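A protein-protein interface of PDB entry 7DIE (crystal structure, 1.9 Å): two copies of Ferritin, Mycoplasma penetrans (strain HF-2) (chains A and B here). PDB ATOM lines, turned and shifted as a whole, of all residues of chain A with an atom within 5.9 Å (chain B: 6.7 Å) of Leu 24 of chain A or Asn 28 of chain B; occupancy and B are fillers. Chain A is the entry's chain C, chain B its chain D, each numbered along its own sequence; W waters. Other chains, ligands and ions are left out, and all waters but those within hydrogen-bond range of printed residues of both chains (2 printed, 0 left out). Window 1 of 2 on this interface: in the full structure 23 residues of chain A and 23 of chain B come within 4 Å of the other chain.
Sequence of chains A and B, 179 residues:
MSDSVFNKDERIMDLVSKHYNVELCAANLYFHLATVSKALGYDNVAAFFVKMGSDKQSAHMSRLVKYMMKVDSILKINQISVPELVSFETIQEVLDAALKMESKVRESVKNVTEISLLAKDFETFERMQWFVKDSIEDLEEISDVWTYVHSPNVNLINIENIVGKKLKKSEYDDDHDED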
ATOM      1  N   HIS A  19      10.057 -27.672  -1.472  1.00  0.00           N
ATOM      2  CA  HIS A  19       9.679 -26.866  -0.320  1.00  0.00           C
ATOM      3  C   HIS A  19       8.204 -26.481  -0.376  1.00  0.00           C
ATOM      4  O   HIS A  19       7.540 -26.435   0.663  1.00  0.00           O
ATOM      5  CB  HIS A  19      10.546 -25.617  -0.176  1.00  0.00           C
ATOM      6  CG  HIS A  19      10.177 -24.830   1.040  1.00  0.00           C
ATOM      7  ND1 HIS A  19      10.392 -25.312   2.314  1.00  0.00           N
ATOM      8  CD2 HIS A  19       9.499 -23.666   1.183  1.00  0.00           C
ATOM      9  CE1 HIS A  19       9.886 -24.465   3.194  1.00  0.00           C
ATOM     10  NE2 HIS A  19       9.348 -23.450   2.533  1.00  0.00           N
ATOM     11  N   TYR A  20       7.663 -26.233  -1.575  1.00  0.00           N
ATOM     12  CA  TYR A  20       6.217 -26.032  -1.675  1.00  0.00           C
ATOM     13  C   TYR A  20       5.469 -27.226  -1.082  1.00  0.00           C
ATOM     14  O   TYR A  20       4.492 -27.052  -0.342  1.00  0.00           O
ATOM     15  CB  TYR A  20       5.813 -25.793  -3.134  1.00  0.00           C
ATOM     16  CG  TYR A  20       4.323 -25.544  -3.363  1.00  0.00           C
ATOM     17  CD1 TYR A  20       3.397 -26.585  -3.263  1.00  0.00           C
ATOM     18  CD2 TYR A  20       3.851 -24.278  -3.706  1.00  0.00           C
ATOM     19  CE1 TYR A  20       2.040 -26.379  -3.463  1.00  0.00           C
ATOM     20  CE2 TYR A  20       2.488 -24.056  -3.927  1.00  0.00           C
ATOM     21  CZ  TYR A  20       1.589 -25.121  -3.802  1.00  0.00           C
ATOM     22  OH  TYR A  20       0.235 -24.942  -4.009  1.00  0.00           O
ATOM     23  N   ASN A  21       5.931 -28.451  -1.378  1.00  0.00           N
ATOM     24  CA  ASN A  21       5.277 -29.632  -0.820  1.00  0.00           C
ATOM     25  C   ASN A  21       5.418 -29.702   0.696  1.00  0.00           C
ATOM     26  O   ASN A  21       4.536 -30.247   1.368  1.00  0.00           O
ATOM     27  CB  ASN A  21       5.833 -30.907  -1.469  1.00  0.00           C
ATOM     28  CG  ASN A  21       5.268 -31.150  -2.865  1.00  0.00           C
ATOM     29  OD1 ASN A  21       4.273 -31.851  -3.030  1.00  0.00           O
ATOM     30  ND2 ASN A  21       5.910 -30.574  -3.876  1.00  0.00           N
ATOM     31  N   VAL A  22       6.518 -29.186   1.253  1.00  0.00           N
ATOM     32  CA  VAL A  22       6.689 -29.186   2.705  1.00  0.00           C
ATOM     33  C   VAL A  22       5.742 -28.182   3.366  1.00  0.00           C
ATOM     34  O   VAL A  22       5.186 -28.446   4.449  1.00  0.00           O
ATOM     35  CB  VAL A  22       8.160 -28.895   3.060  1.00  0.00           C
ATOM     36  CG1 VAL A  22       8.317 -28.647   4.563  1.00  0.00           C
ATOM     37  CG2 VAL A  22       9.071 -30.047   2.614  1.00  0.00           C
ATOM     38  N   GLU A  23       5.552 -27.008   2.741  1.00  0.00           N
ATOM     39  CA  GLU A  23       4.585 -26.047   3.281  1.00  0.00           C
ATOM     40  C   GLU A  23       3.163 -26.588   3.179  1.00  0.00           C
ATOM     41  O   GLU A  23       2.330 -26.361   4.074  1.00  0.00           O
ATOM     42  CB  GLU A  23       4.684 -24.705   2.533  1.00  0.00           C
ATOM     43  CG  GLU A  23       6.069 -24.037   2.575  1.00  0.00           C
ATOM     44  CD  GLU A  23       6.293 -23.162   3.807  1.00  0.00           C
ATOM     45  OE1 GLU A  23       5.553 -23.298   4.803  1.00  0.00           O
ATOM     46  OE2 GLU A  23       7.229 -22.333   3.790  1.00  0.00           O
ATOM     47  N   LEU A  24       2.858 -27.274   2.073  1.00  0.00           N
ATOM     48  CA  LEU A  24       1.538 -27.879   1.914  1.00  0.00           C
ATOM     49  C   LEU A  24       1.347 -29.033   2.888  1.00  0.00           C
ATOM     50  O   LEU A  24       0.259 -29.207   3.453  1.00  0.00           O
ATOM     51  CB  LEU A  24       1.347 -28.353   0.465  1.00  0.00           C
ATOM     52  CG  LEU A  24       0.070 -29.154   0.156  1.00  0.00           C
ATOM     53  CD1 LEU A  24      -1.209 -28.385   0.581  1.00  0.00           C
ATOM     54  CD2 LEU A  24       0.038 -29.488  -1.333  1.00  0.00           C
ATOM     55  N   CYS A  25       2.396 -29.832   3.098  1.00  0.00           N
ATOM     56  CA  CYS A  25       2.345 -30.855   4.141  1.00  0.00           C
ATOM     57  C   CYS A  25       1.984 -30.242   5.488  1.00  0.00           C
ATOM     58  O   CYS A  25       1.137 -30.777   6.216  1.00  0.00           O
ATOM     59  CB  CYS A  25       3.686 -31.591   4.225  1.00  0.00           C
ATOM     60  SG  CYS A  25       3.645 -33.014   5.360  1.00  0.00           S
ATOM     61  N   ALA A  26       2.615 -29.110   5.837  1.00  0.00           N
ATOM     62  CA  ALA A  26       2.277 -28.422   7.081  1.00  0.00           C
ATOM     63  C   ALA A  26       0.822 -27.952   7.077  1.00  0.00           C
ATOM     64  O   ALA A  26       0.089 -28.161   8.054  1.00  0.00           O
ATOM     65  CB  ALA A  26       3.235 -27.245   7.304  1.00  0.00           C
ATOM     66  N   ALA A  27       0.384 -27.310   5.990  1.00  0.00           N
ATOM     67  CA  ALA A  27      -1.015 -26.878   5.910  1.00  0.00           C
ATOM     68  C   ALA A  27      -1.962 -28.061   6.081  1.00  0.00           C
ATOM     69  O   ALA A  27      -2.927 -27.999   6.858  1.00  0.00           O
ATOM     70  CB  ALA A  27      -1.283 -26.171   4.575  1.00  0.00           C
ATOM     71  N   ASN A  28      -1.692 -29.156   5.358  1.00  0.00           N
ATOM     72  CA  ASN A  28      -2.524 -30.350   5.458  1.00  0.00           C
ATOM     73  C   ASN A  28      -2.545 -30.886   6.880  1.00  0.00           C
ATOM     74  O   ASN A  28      -3.602 -31.285   7.380  1.00  0.00           O
ATOM     75  CB  ASN A  28      -2.025 -31.435   4.494  1.00  0.00           C
ATOM     76  CG  ASN A  28      -2.411 -31.164   3.059  1.00  0.00           C
ATOM     77  OD1 ASN A  28      -3.432 -30.514   2.785  1.00  0.00           O
ATOM     78  ND2 ASN A  28      -1.606 -31.681   2.121  1.00  0.00           N
ATOM     79  N   LEU A  29      -1.383 -30.915   7.546  1.00  0.00           N
ATOM     80  CA  LEU A  29      -1.359 -31.345   8.939  1.00  0.00           C
ATOM     81  C   LEU A  29      -2.167 -30.401   9.822  1.00  0.00           C
ATOM     82  O   LEU A  29      -2.934 -30.850  10.686  1.00  0.00           O
ATOM     83  CB  LEU A  29       0.080 -31.448   9.446  1.00  0.00           C
ATOM     84  CG  LEU A  29       0.130 -31.908  10.909  1.00  0.00           C
ATOM     85  CD1 LEU A  29      -0.396 -33.359  11.077  1.00  0.00           C
ATOM     86  CD2 LEU A  29       1.520 -31.746  11.544  1.00  0.00           C
ATOM     87  N   LYS A  56      -0.275 -20.686   5.522  1.00  0.00           N
ATOM     88  CA  LYS A  56       0.612 -21.434   4.625  1.00  0.00           C
ATOM     89  C   LYS A  56       0.126 -21.333   3.183  1.00  0.00           C
ATOM     90  O   LYS A  56       0.923 -21.143   2.257  1.00  0.00           O
ATOM     91  CB  LYS A  56       0.702 -22.908   5.035  1.00  0.00           C
ATOM     92  CG  LYS A  56       1.436 -23.166   6.368  1.00  0.00           C
ATOM     93  CD  LYS A  56       2.826 -22.516   6.398  1.00  0.00           C
ATOM     94  CE  LYS A  56       3.643 -23.054   7.610  1.00  0.00           C
ATOM     95  NZ  LYS A  56       4.971 -22.352   7.695  1.00  0.00           N
ATOM     96  N   MET A  61       2.699 -20.840   0.116  1.00  0.00           N
ATOM     97  CA  MET A  61       2.530 -21.529  -1.166  1.00  0.00           C
ATOM     98  C   MET A  61       2.302 -20.537  -2.307  1.00  0.00           C
ATOM     99  O   MET A  61       2.820 -20.726  -3.414  1.00  0.00           O
ATOM    100  CB  MET A  61       1.375 -22.524  -1.058  1.00  0.00           C
ATOM    101  CG  MET A  61       1.707 -23.727  -0.141  1.00  0.00           C
ATOM    102  SD  MET A  61       0.255 -24.405   0.715  1.00  0.00           S
ATOM    103  CE  MET A  61      -0.722 -24.823  -0.680  1.00  0.00           C
ATOM    104  N   LEU A  75       5.920 -26.529 -11.121  1.00  0.00           N
ATOM    105  CA  LEU A  75       5.618 -26.978  -9.767  1.00  0.00           C
ATOM    106  C   LEU A  75       5.081 -28.403  -9.811  1.00  0.00           C
ATOM    107  O   LEU A  75       4.094 -28.679 -10.497  1.00  0.00           O
ATOM    108  CB  LEU A  75       4.576 -26.067  -9.105  1.00  0.00           C
ATOM    109  CG  LEU A  75       3.961 -26.584  -7.798  1.00  0.00           C
ATOM    110  CD1 LEU A  75       5.030 -26.679  -6.705  1.00  0.00           C
ATOM    111  CD2 LEU A  75       2.833 -25.638  -7.363  1.00  0.00           C
ATOM    112  N   ILE A  77       3.542 -31.384  -7.476  1.00  0.00           N
ATOM    113  CA  ILE A  77       2.996 -31.836  -6.202  1.00  0.00           C
ATOM    114  C   ILE A  77       3.164 -33.347  -6.119  1.00  0.00           C
ATOM    115  O   ILE A  77       2.866 -34.059  -7.083  1.00  0.00           O
ATOM    116  CB  ILE A  77       1.513 -31.456  -6.064  1.00  0.00           C
ATOM    117  CG1 ILE A  77       1.297 -29.956  -6.282  1.00  0.00           C
ATOM    118  CG2 ILE A  77       0.962 -31.966  -4.726  1.00  0.00           C
ATOM    119  CD1 ILE A  77       2.200 -29.106  -5.513  1.00  0.00           C
ATOM    120  N   SER A  81       3.719 -33.969   0.173  1.00  0.00           N
ATOM    121  CA  SER A  81       2.694 -33.056   0.668  1.00  0.00           C
ATOM    122  C   SER A  81       1.698 -33.716   1.606  1.00  0.00           C
ATOM    123  O   SER A  81       0.865 -33.013   2.180  1.00  0.00           O
ATOM    124  CB  SER A  81       1.934 -32.442  -0.513  1.00  0.00           C
ATOM    125  OG  SER A  81       1.143 -33.422  -1.180  1.00  0.00           O
ATOM    126  N   PRO A  83       0.864 -35.549   5.004  1.00  0.00           N
ATOM    127  CA  PRO A  83       1.489 -35.802   6.306  1.00  0.00           C
ATOM    128  C   PRO A  83       1.279 -37.238   6.764  1.00  0.00           C
ATOM    129  O   PRO A  83       0.256 -37.865   6.473  1.00  0.00           O
ATOM    130  CB  PRO A  83       0.792 -34.802   7.239  1.00  0.00           C
ATOM    131  CG  PRO A  83      -0.462 -34.438   6.547  1.00  0.00           C
ATOM    132  CD  PRO A  83      -0.202 -34.538   5.080  1.00  0.00           C
ATOM    133  N   ASN B  21     -10.349 -34.109  -0.040  1.00  0.00           N
ATOM    134  CA  ASN B  21      -9.162 -34.524  -0.783  1.00  0.00           C
ATOM    135  C   ASN B  21      -9.346 -34.355  -2.288  1.00  0.00           C
ATOM    136  O   ASN B  21      -8.375 -34.087  -2.998  1.00  0.00           O
ATOM    137  CB  ASN B  21      -8.806 -35.982  -0.454  1.00  0.00           C
ATOM    138  CG  ASN B  21      -8.111 -36.131   0.879  1.00  0.00           C
ATOM    139  OD1 ASN B  21      -6.890 -36.144   0.948  1.00  0.00           O
ATOM    140  ND2 ASN B  21      -8.889 -36.250   1.955  1.00  0.00           N
ATOM    141  N   GLU B  23     -11.270 -31.944  -3.740  1.00  0.00           N
ATOM    142  CA  GLU B  23     -11.121 -30.510  -4.010  1.00  0.00           C
ATOM    143  C   GLU B  23      -9.652 -30.103  -3.942  1.00  0.00           C
ATOM    144  O   GLU B  23      -9.180 -29.269  -4.740  1.00  0.00           O
ATOM    145  CB  GLU B  23     -11.948 -29.670  -3.013  1.00  0.00           C
ATOM    146  CG  GLU B  23     -13.489 -29.950  -2.989  1.00  0.00           C
ATOM    147  CD  GLU B  23     -14.269 -29.164  -4.039  1.00  0.00           C
ATOM    148  OE1 GLU B  23     -13.644 -28.609  -4.965  1.00  0.00           O
ATOM    149  OE2 GLU B  23     -15.522 -29.112  -3.970  1.00  0.00           O
ATOM    150  N   LEU B  24      -8.921 -30.668  -2.979  1.00  0.00           N
ATOM    151  CA  LEU B  24      -7.492 -30.392  -2.849  1.00  0.00           C
ATOM    152  C   LEU B  24      -6.711 -30.973  -4.020  1.00  0.00           C
ATOM    153  O   LEU B  24      -5.738 -30.366  -4.487  1.00  0.00           O
ATOM    154  CB  LEU B  24      -6.973 -30.948  -1.513  1.00  0.00           C
ATOM    155  CG  LEU B  24      -5.467 -30.885  -1.268  1.00  0.00           C
ATOM    156  CD1 LEU B  24      -4.931 -29.437  -1.452  1.00  0.00           C
ATOM    157  CD2 LEU B  24      -5.107 -31.451   0.116  1.00  0.00           C
ATOM    158  N   CYS B  25      -7.115 -32.147  -4.509  1.00  0.00           N
ATOM    159  CA  CYS B  25      -6.493 -32.683  -5.714  1.00  0.00           C
ATOM    160  C   CYS B  25      -6.656 -31.714  -6.877  1.00  0.00           C
ATOM    161  O   CYS B  25      -5.703 -31.456  -7.616  1.00  0.00           O
ATOM    162  CB  CYS B  25      -7.101 -34.051  -6.046  1.00  0.00           C
ATOM    163  SG  CYS B  25      -6.307 -34.887  -7.423  1.00  0.00           S
ATOM    164  N   ALA B  26      -7.861 -31.142  -7.034  1.00  0.00           N
ATOM    165  CA  ALA B  26      -8.087 -30.141  -8.070  1.00  0.00           C
ATOM    166  C   ALA B  26      -7.196 -28.921  -7.856  1.00  0.00           C
ATOM    167  O   ALA B  26      -6.560 -28.436  -8.796  1.00  0.00           O
ATOM    168  CB  ALA B  26      -9.563 -29.729  -8.092  1.00  0.00           C
ATOM    169  N   ALA B  27      -7.136 -28.414  -6.621  1.00  0.00           N
ATOM    170  CA  ALA B  27      -6.292 -27.249  -6.337  1.00  0.00           C
ATOM    171  C   ALA B  27      -4.843 -27.538  -6.700  1.00  0.00           C
ATOM    172  O   ALA B  27      -4.188 -26.744  -7.393  1.00  0.00           O
ATOM    173  CB  ALA B  27      -6.397 -26.862  -4.856  1.00  0.00           C
ATOM    174  N   ASN B  28      -4.334 -28.687  -6.238  1.00  0.00           N
ATOM    175  CA  ASN B  28      -2.971 -29.112  -6.550  1.00  0.00           C
ATOM    176  C   ASN B  28      -2.753 -29.207  -8.053  1.00  0.00           C
ATOM    177  O   ASN B  28      -1.746 -28.715  -8.579  1.00  0.00           O
ATOM    178  CB  ASN B  28      -2.676 -30.463  -5.869  1.00  0.00           C
ATOM    179  CG  ASN B  28      -2.446 -30.318  -4.364  1.00  0.00           C
ATOM    180  OD1 ASN B  28      -2.027 -29.262  -3.891  1.00  0.00           O
ATOM    181  ND2 ASN B  28      -2.722 -31.385  -3.605  1.00  0.00           N
ATOM    182  N   LEU B  29      -3.695 -29.825  -8.771  1.00  0.00           N
ATOM    183  CA  LEU B  29      -3.551 -29.885 -10.221  1.00  0.00           C
ATOM    184  C   LEU B  29      -3.525 -28.485 -10.824  1.00  0.00           C
ATOM    185  O   LEU B  29      -2.698 -28.194 -11.693  1.00  0.00           O
ATOM    186  CB  LEU B  29      -4.685 -30.704 -10.842  1.00  0.00           C
ATOM    187  CG  LEU B  29      -4.598 -30.747 -12.376  1.00  0.00           C
ATOM    188  CD1 LEU B  29      -3.334 -31.456 -12.864  1.00  0.00           C
ATOM    189  CD2 LEU B  29      -5.839 -31.390 -12.990  1.00  0.00           C
ATOM    190  N   TYR B  30      -4.432 -27.599 -10.380  1.00  0.00           N
ATOM    191  CA  TYR B  30      -4.517 -26.278 -11.005  1.00  0.00           C
ATOM    192  C   TYR B  30      -3.256 -25.462 -10.743  1.00  0.00           C
ATOM    193  O   TYR B  30      -2.791 -24.748 -11.631  1.00  0.00           O
ATOM    194  CB  TYR B  30      -5.774 -25.512 -10.535  1.00  0.00           C
ATOM    195  CG  TYR B  30      -7.068 -26.237 -10.873  1.00  0.00           C
ATOM    196  CD1 TYR B  30      -7.113 -27.140 -11.933  1.00  0.00           C
ATOM    197  CD2 TYR B  30      -8.230 -26.043 -10.121  1.00  0.00           C
ATOM    198  CE1 TYR B  30      -8.275 -27.838 -12.240  1.00  0.00           C
ATOM    199  CE2 TYR B  30      -9.412 -26.737 -10.421  1.00  0.00           C
ATOM    200  CZ  TYR B  30      -9.419 -27.643 -11.491  1.00  0.00           C
ATOM    201  OH  TYR B  30     -10.563 -28.359 -11.811  1.00  0.00           O
ATOM    202  N   PHE B  31      -2.673 -25.560  -9.547  1.00  0.00           N
ATOM    203  CA  PHE B  31      -1.418 -24.844  -9.331  1.00  0.00           C
ATOM    204  C   PHE B  31      -0.299 -25.415 -10.199  1.00  0.00           C
ATOM    205  O   PHE B  31       0.514 -24.662 -10.744  1.00  0.00           O
ATOM    206  CB  PHE B  31      -1.055 -24.858  -7.843  1.00  0.00           C
ATOM    207  CG  PHE B  31      -1.961 -23.986  -6.996  1.00  0.00           C
ATOM    208  CD1 PHE B  31      -2.131 -22.640  -7.300  1.00  0.00           C
ATOM    209  CD2 PHE B  31      -2.657 -24.520  -5.915  1.00  0.00           C
ATOM    210  CE1 PHE B  31      -2.975 -21.830  -6.527  1.00  0.00           C
ATOM    211  CE2 PHE B  31      -3.508 -23.717  -5.139  1.00  0.00           C
ATOM    212  CZ  PHE B  31      -3.659 -22.375  -5.450  1.00  0.00           C
ATOM    213  N   HIS B  32      -0.259 -26.742 -10.374  1.00  0.00           N
ATOM    214  CA  HIS B  32       0.666 -27.335 -11.346  1.00  0.00           C
ATOM    215  C   HIS B  32       0.402 -26.812 -12.760  1.00  0.00           C
ATOM    216  O   HIS B  32       1.329 -26.387 -13.463  1.00  0.00           O
ATOM    217  CB  HIS B  32       0.558 -28.866 -11.301  1.00  0.00           C
ATOM    218  CG  HIS B  32       1.210 -29.553 -12.463  1.00  0.00           C
ATOM    219  ND1 HIS B  32       2.578 -29.694 -12.574  1.00  0.00           N
ATOM    220  CD2 HIS B  32       0.679 -30.147 -13.558  1.00  0.00           C
ATOM    221  CE1 HIS B  32       2.862 -30.340 -13.695  1.00  0.00           C
ATOM    222  NE2 HIS B  32       1.728 -30.627 -14.309  1.00  0.00           N
ATOM    223  N   LEU B  33      -0.865 -26.823 -13.190  1.00  0.00           N
ATOM    224  CA  LEU B  33      -1.200 -26.400 -14.552  1.00  0.00           C
ATOM    225  C   LEU B  33      -0.943 -24.914 -14.775  1.00  0.00           C
ATOM    226  O   LEU B  33      -0.702 -24.488 -15.911  1.00  0.00           O
ATOM    227  CB  LEU B  33      -2.660 -26.727 -14.863  1.00  0.00           C
ATOM    228  CG  LEU B  33      -2.999 -28.218 -14.895  1.00  0.00           C
ATOM    229  CD1 LEU B  33      -4.455 -28.424 -15.278  1.00  0.00           C
ATOM    230  CD2 LEU B  33      -2.066 -28.953 -15.858  1.00  0.00           C
ATOM    231  N   GLY B  53      -7.431 -22.594  -8.351  1.00  0.00           N
ATOM    232  CA  GLY B  53      -6.874 -23.293  -7.201  1.00  0.00           C
ATOM    233  C   GLY B  53      -7.074 -22.528  -5.902  1.00  0.00           C
ATOM    234  O   GLY B  53      -7.349 -23.122  -4.857  1.00  0.00           O
ATOM    235  N   GLN B  57      -9.305 -23.555  -2.318  1.00  0.00           N
ATOM    236  CA  GLN B  57      -8.836 -23.399  -0.940  1.00  0.00           C
ATOM    237  C   GLN B  57      -9.797 -22.555  -0.116  1.00  0.00           C
ATOM    238  O   GLN B  57     -10.220 -22.957   0.979  1.00  0.00           O
ATOM    239  CB  GLN B  57      -7.453 -22.745  -0.923  1.00  0.00           C
ATOM    240  CG  GLN B  57      -6.338 -23.502  -1.592  1.00  0.00           C
ATOM    241  CD  GLN B  57      -5.103 -22.638  -1.734  1.00  0.00           C
ATOM    242  OE1 GLN B  57      -5.206 -21.424  -1.891  1.00  0.00           O
ATOM    243  NE2 GLN B  57      -3.936 -23.251  -1.649  1.00  0.00           N
ATOM    244  N   MET B  61     -12.561 -26.041   0.288  1.00  0.00           N
ATOM    245  CA  MET B  61     -11.891 -26.699   1.403  1.00  0.00           C
ATOM    246  C   MET B  61     -12.243 -26.046   2.738  1.00  0.00           C
ATOM    247  O   MET B  61     -12.472 -26.737   3.737  1.00  0.00           O
ATOM    248  CB  MET B  61     -10.382 -26.683   1.162  1.00  0.00           C
ATOM    249  CG  MET B  61      -9.969 -27.641   0.018  1.00  0.00           C
ATOM    250  SD  MET B  61      -8.424 -27.166  -0.787  1.00  0.00           S
ATOM    251  CE  MET B  61      -7.352 -27.066   0.614  1.00  0.00           C
ATOM    252  N   SER B  81      -5.406 -36.760  -2.533  1.00  0.00           N
ATOM    253  CA  SER B  81      -5.189 -35.336  -2.792  1.00  0.00           C
ATOM    254  C   SER B  81      -4.076 -35.059  -3.789  1.00  0.00           C
ATOM    255  O   SER B  81      -3.904 -33.902  -4.185  1.00  0.00           O
ATOM    256  CB  SER B  81      -4.855 -34.618  -1.486  1.00  0.00           C
ATOM    257  OG  SER B  81      -3.579 -35.044  -1.010  1.00  0.00           O
ATOM    258  N   VAL B  82      -3.292 -36.060  -4.172  1.00  0.00           N
ATOM    259  CA  VAL B  82      -2.131 -35.864  -5.033  1.00  0.00           C
ATOM    260  C   VAL B  82      -2.544 -36.193  -6.462  1.00  0.00           C
ATOM    261  O   VAL B  82      -2.920 -37.346  -6.729  1.00  0.00           O
ATOM    262  CB  VAL B  82      -0.952 -36.743  -4.594  1.00  0.00           C
ATOM    263  CG1 VAL B  82       0.221 -36.553  -5.534  1.00  0.00           C
ATOM    264  CG2 VAL B  82      -0.574 -36.431  -3.142  1.00  0.00           C
ATOM    265  N   PRO B  83      -2.500 -35.240  -7.395  1.00  0.00           N
ATOM    266  CA  PRO B  83      -2.925 -35.544  -8.763  1.00  0.00           C
ATOM    267  C   PRO B  83      -1.921 -36.427  -9.492  1.00  0.00           C
ATOM    268  O   PRO B  83      -0.711 -36.372  -9.260  1.00  0.00           O
ATOM    269  CB  PRO B  83      -3.042 -34.162  -9.426  1.00  0.00           C
ATOM    270  CG  PRO B  83      -2.256 -33.234  -8.558  1.00  0.00           C
ATOM    271  CD  PRO B  83      -2.302 -33.792  -7.181  1.00  0.00           C
ATOM    272  N   LEU B  85      -0.011 -36.806 -12.555  1.00  0.00           N
ATOM    273  CA  LEU B  85       0.459 -35.893 -13.593  1.00  0.00           C
ATOM    274  C   LEU B  85       0.970 -36.654 -14.812  1.00  0.00           C
ATOM    275  O   LEU B  85       1.696 -37.645 -14.690  1.00  0.00           O
ATOM    276  CB  LEU B  85       1.565 -34.980 -13.059  1.00  0.00           C
ATOM    277  CG  LEU B  85       1.218 -34.192 -11.795  1.00  0.00           C
ATOM    278  CD1 LEU B  85       2.347 -33.243 -11.402  1.00  0.00           C
ATOM    279  CD2 LEU B  85      -0.096 -33.442 -11.988  1.00  0.00           C
HETATM  280  O   HOH W   1      -2.067 -26.659  -3.271  1.00  0.00           O
HETATM  281  O   HOH W   2      -1.732 -32.737  -0.861  1.00  0.00           O
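Among the printed residues, pairs that only touch across the chains: Tyr 20 of chain A with Phe 31 of chain B, Leu 24 of chain A with Asn 28 of chain B, Asn 28 of chain A with Leu 24 of chain B, Met 61 of chain A with Gln 57 of chain B, Leu 75 of chain A with Phe 31 of chain B, Ile 77 of chain A with Asn 28 of chain B, Ile 77 of chain A with Val 82 of chain B and Ser 81 of chain A with Val 82 of chain B.
The backbone carbonyl oxygen of Ser 81 of chain B lies within hydrogen-bond range of the side-chain amide nitrogen of Asn 28 of chain B (2.8 Å). The backbone carbonyl oxygen (O) of Leu 24 of chain A lies close to the side-chain amide nitrogen (ND2) of Asn 28 of chain A, 3.4 Å away. The backbone carbonyl oxygen of Lys 56 of chain A is in hydrogen-bond range of the backbone NH of Met 61 of chain A (2.8 Å). The side-chain amide nitrogen of Asn 28 of chain A is in hydrogen-bond range of the backbone carbonyl oxygen of Ser 81 of chain A, at 2.8 Å. The side-chain amide nitrogen of Asn 28 of chain B sits close to the backbone carbonyl oxygen of Leu 24 of chain B, at 3.3 Å.
Leu 24 of chain A touches Asn 28 of chain B, and with the chains exchanged Asn 28 of chain A touches Leu 24 of chain B. Of the 9 pairs that touch across the chains among the printed residues, 2 have their exchanged pair printed and touching as well.
Water W1 bridges OD1 of Asn 28 of chain B (2.7 Å) and OH of Tyr 20 of chain A (3.0 Å). Water W2 lies within hydrogen-bond range of the side-chain hydroxyl of Ser 81 of chain B, the side-chain hydroxyl of Ser 81 of chain A, the side-chain amide nitrogen of Asn 28 of chain A and the side-chain amide nitrogen of Asn 28 of chain B.
O of Leu 75 of chain A lies within hydrogen-bond range of ND1 of His 32 of chain B, 2.8 Å away.
Hydrophobic or aromatic side chains of chain B within 4 Å of the printed part of chain A: Leu 24, Phe 31, His 32 and Val 82. Of the 17 printed residues of chain A, 7 touch a printed residue of chain B. Hydrophobic or aromatic side chains of chain A that line the printed part of chain B: Tyr 20, Leu 24, Met 61, Leu 75 and Ile 77.
Leu 24 of chain A touches one residue of chain B. Of the printed residues of chain B, Asn 28 of chain A touches Leu 24 (3.3 Å). Printed residues of chain B within 4 Å of Ser 81 of chain A: Val 82 (3.98 Å). Cys 25 of chain B touches none of the printed residues of chain A. Asn 28 of chain B touches just these residues of chain A: Leu 24 and Ile 77. Of the printed residues of chain A, Phe 31 of chain B touches Tyr 20 (3.5 Å) and Leu 75 (3.99 Å). Of the printed residues of chain A, His 32 of chain B touches Leu 75 (2.8 Å). Gly 53 of chain B touches none of the printed residues of chain A. Printed residues of chain A within 4 Å of Val 82 of chain B: Ile 77 and Ser 81.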
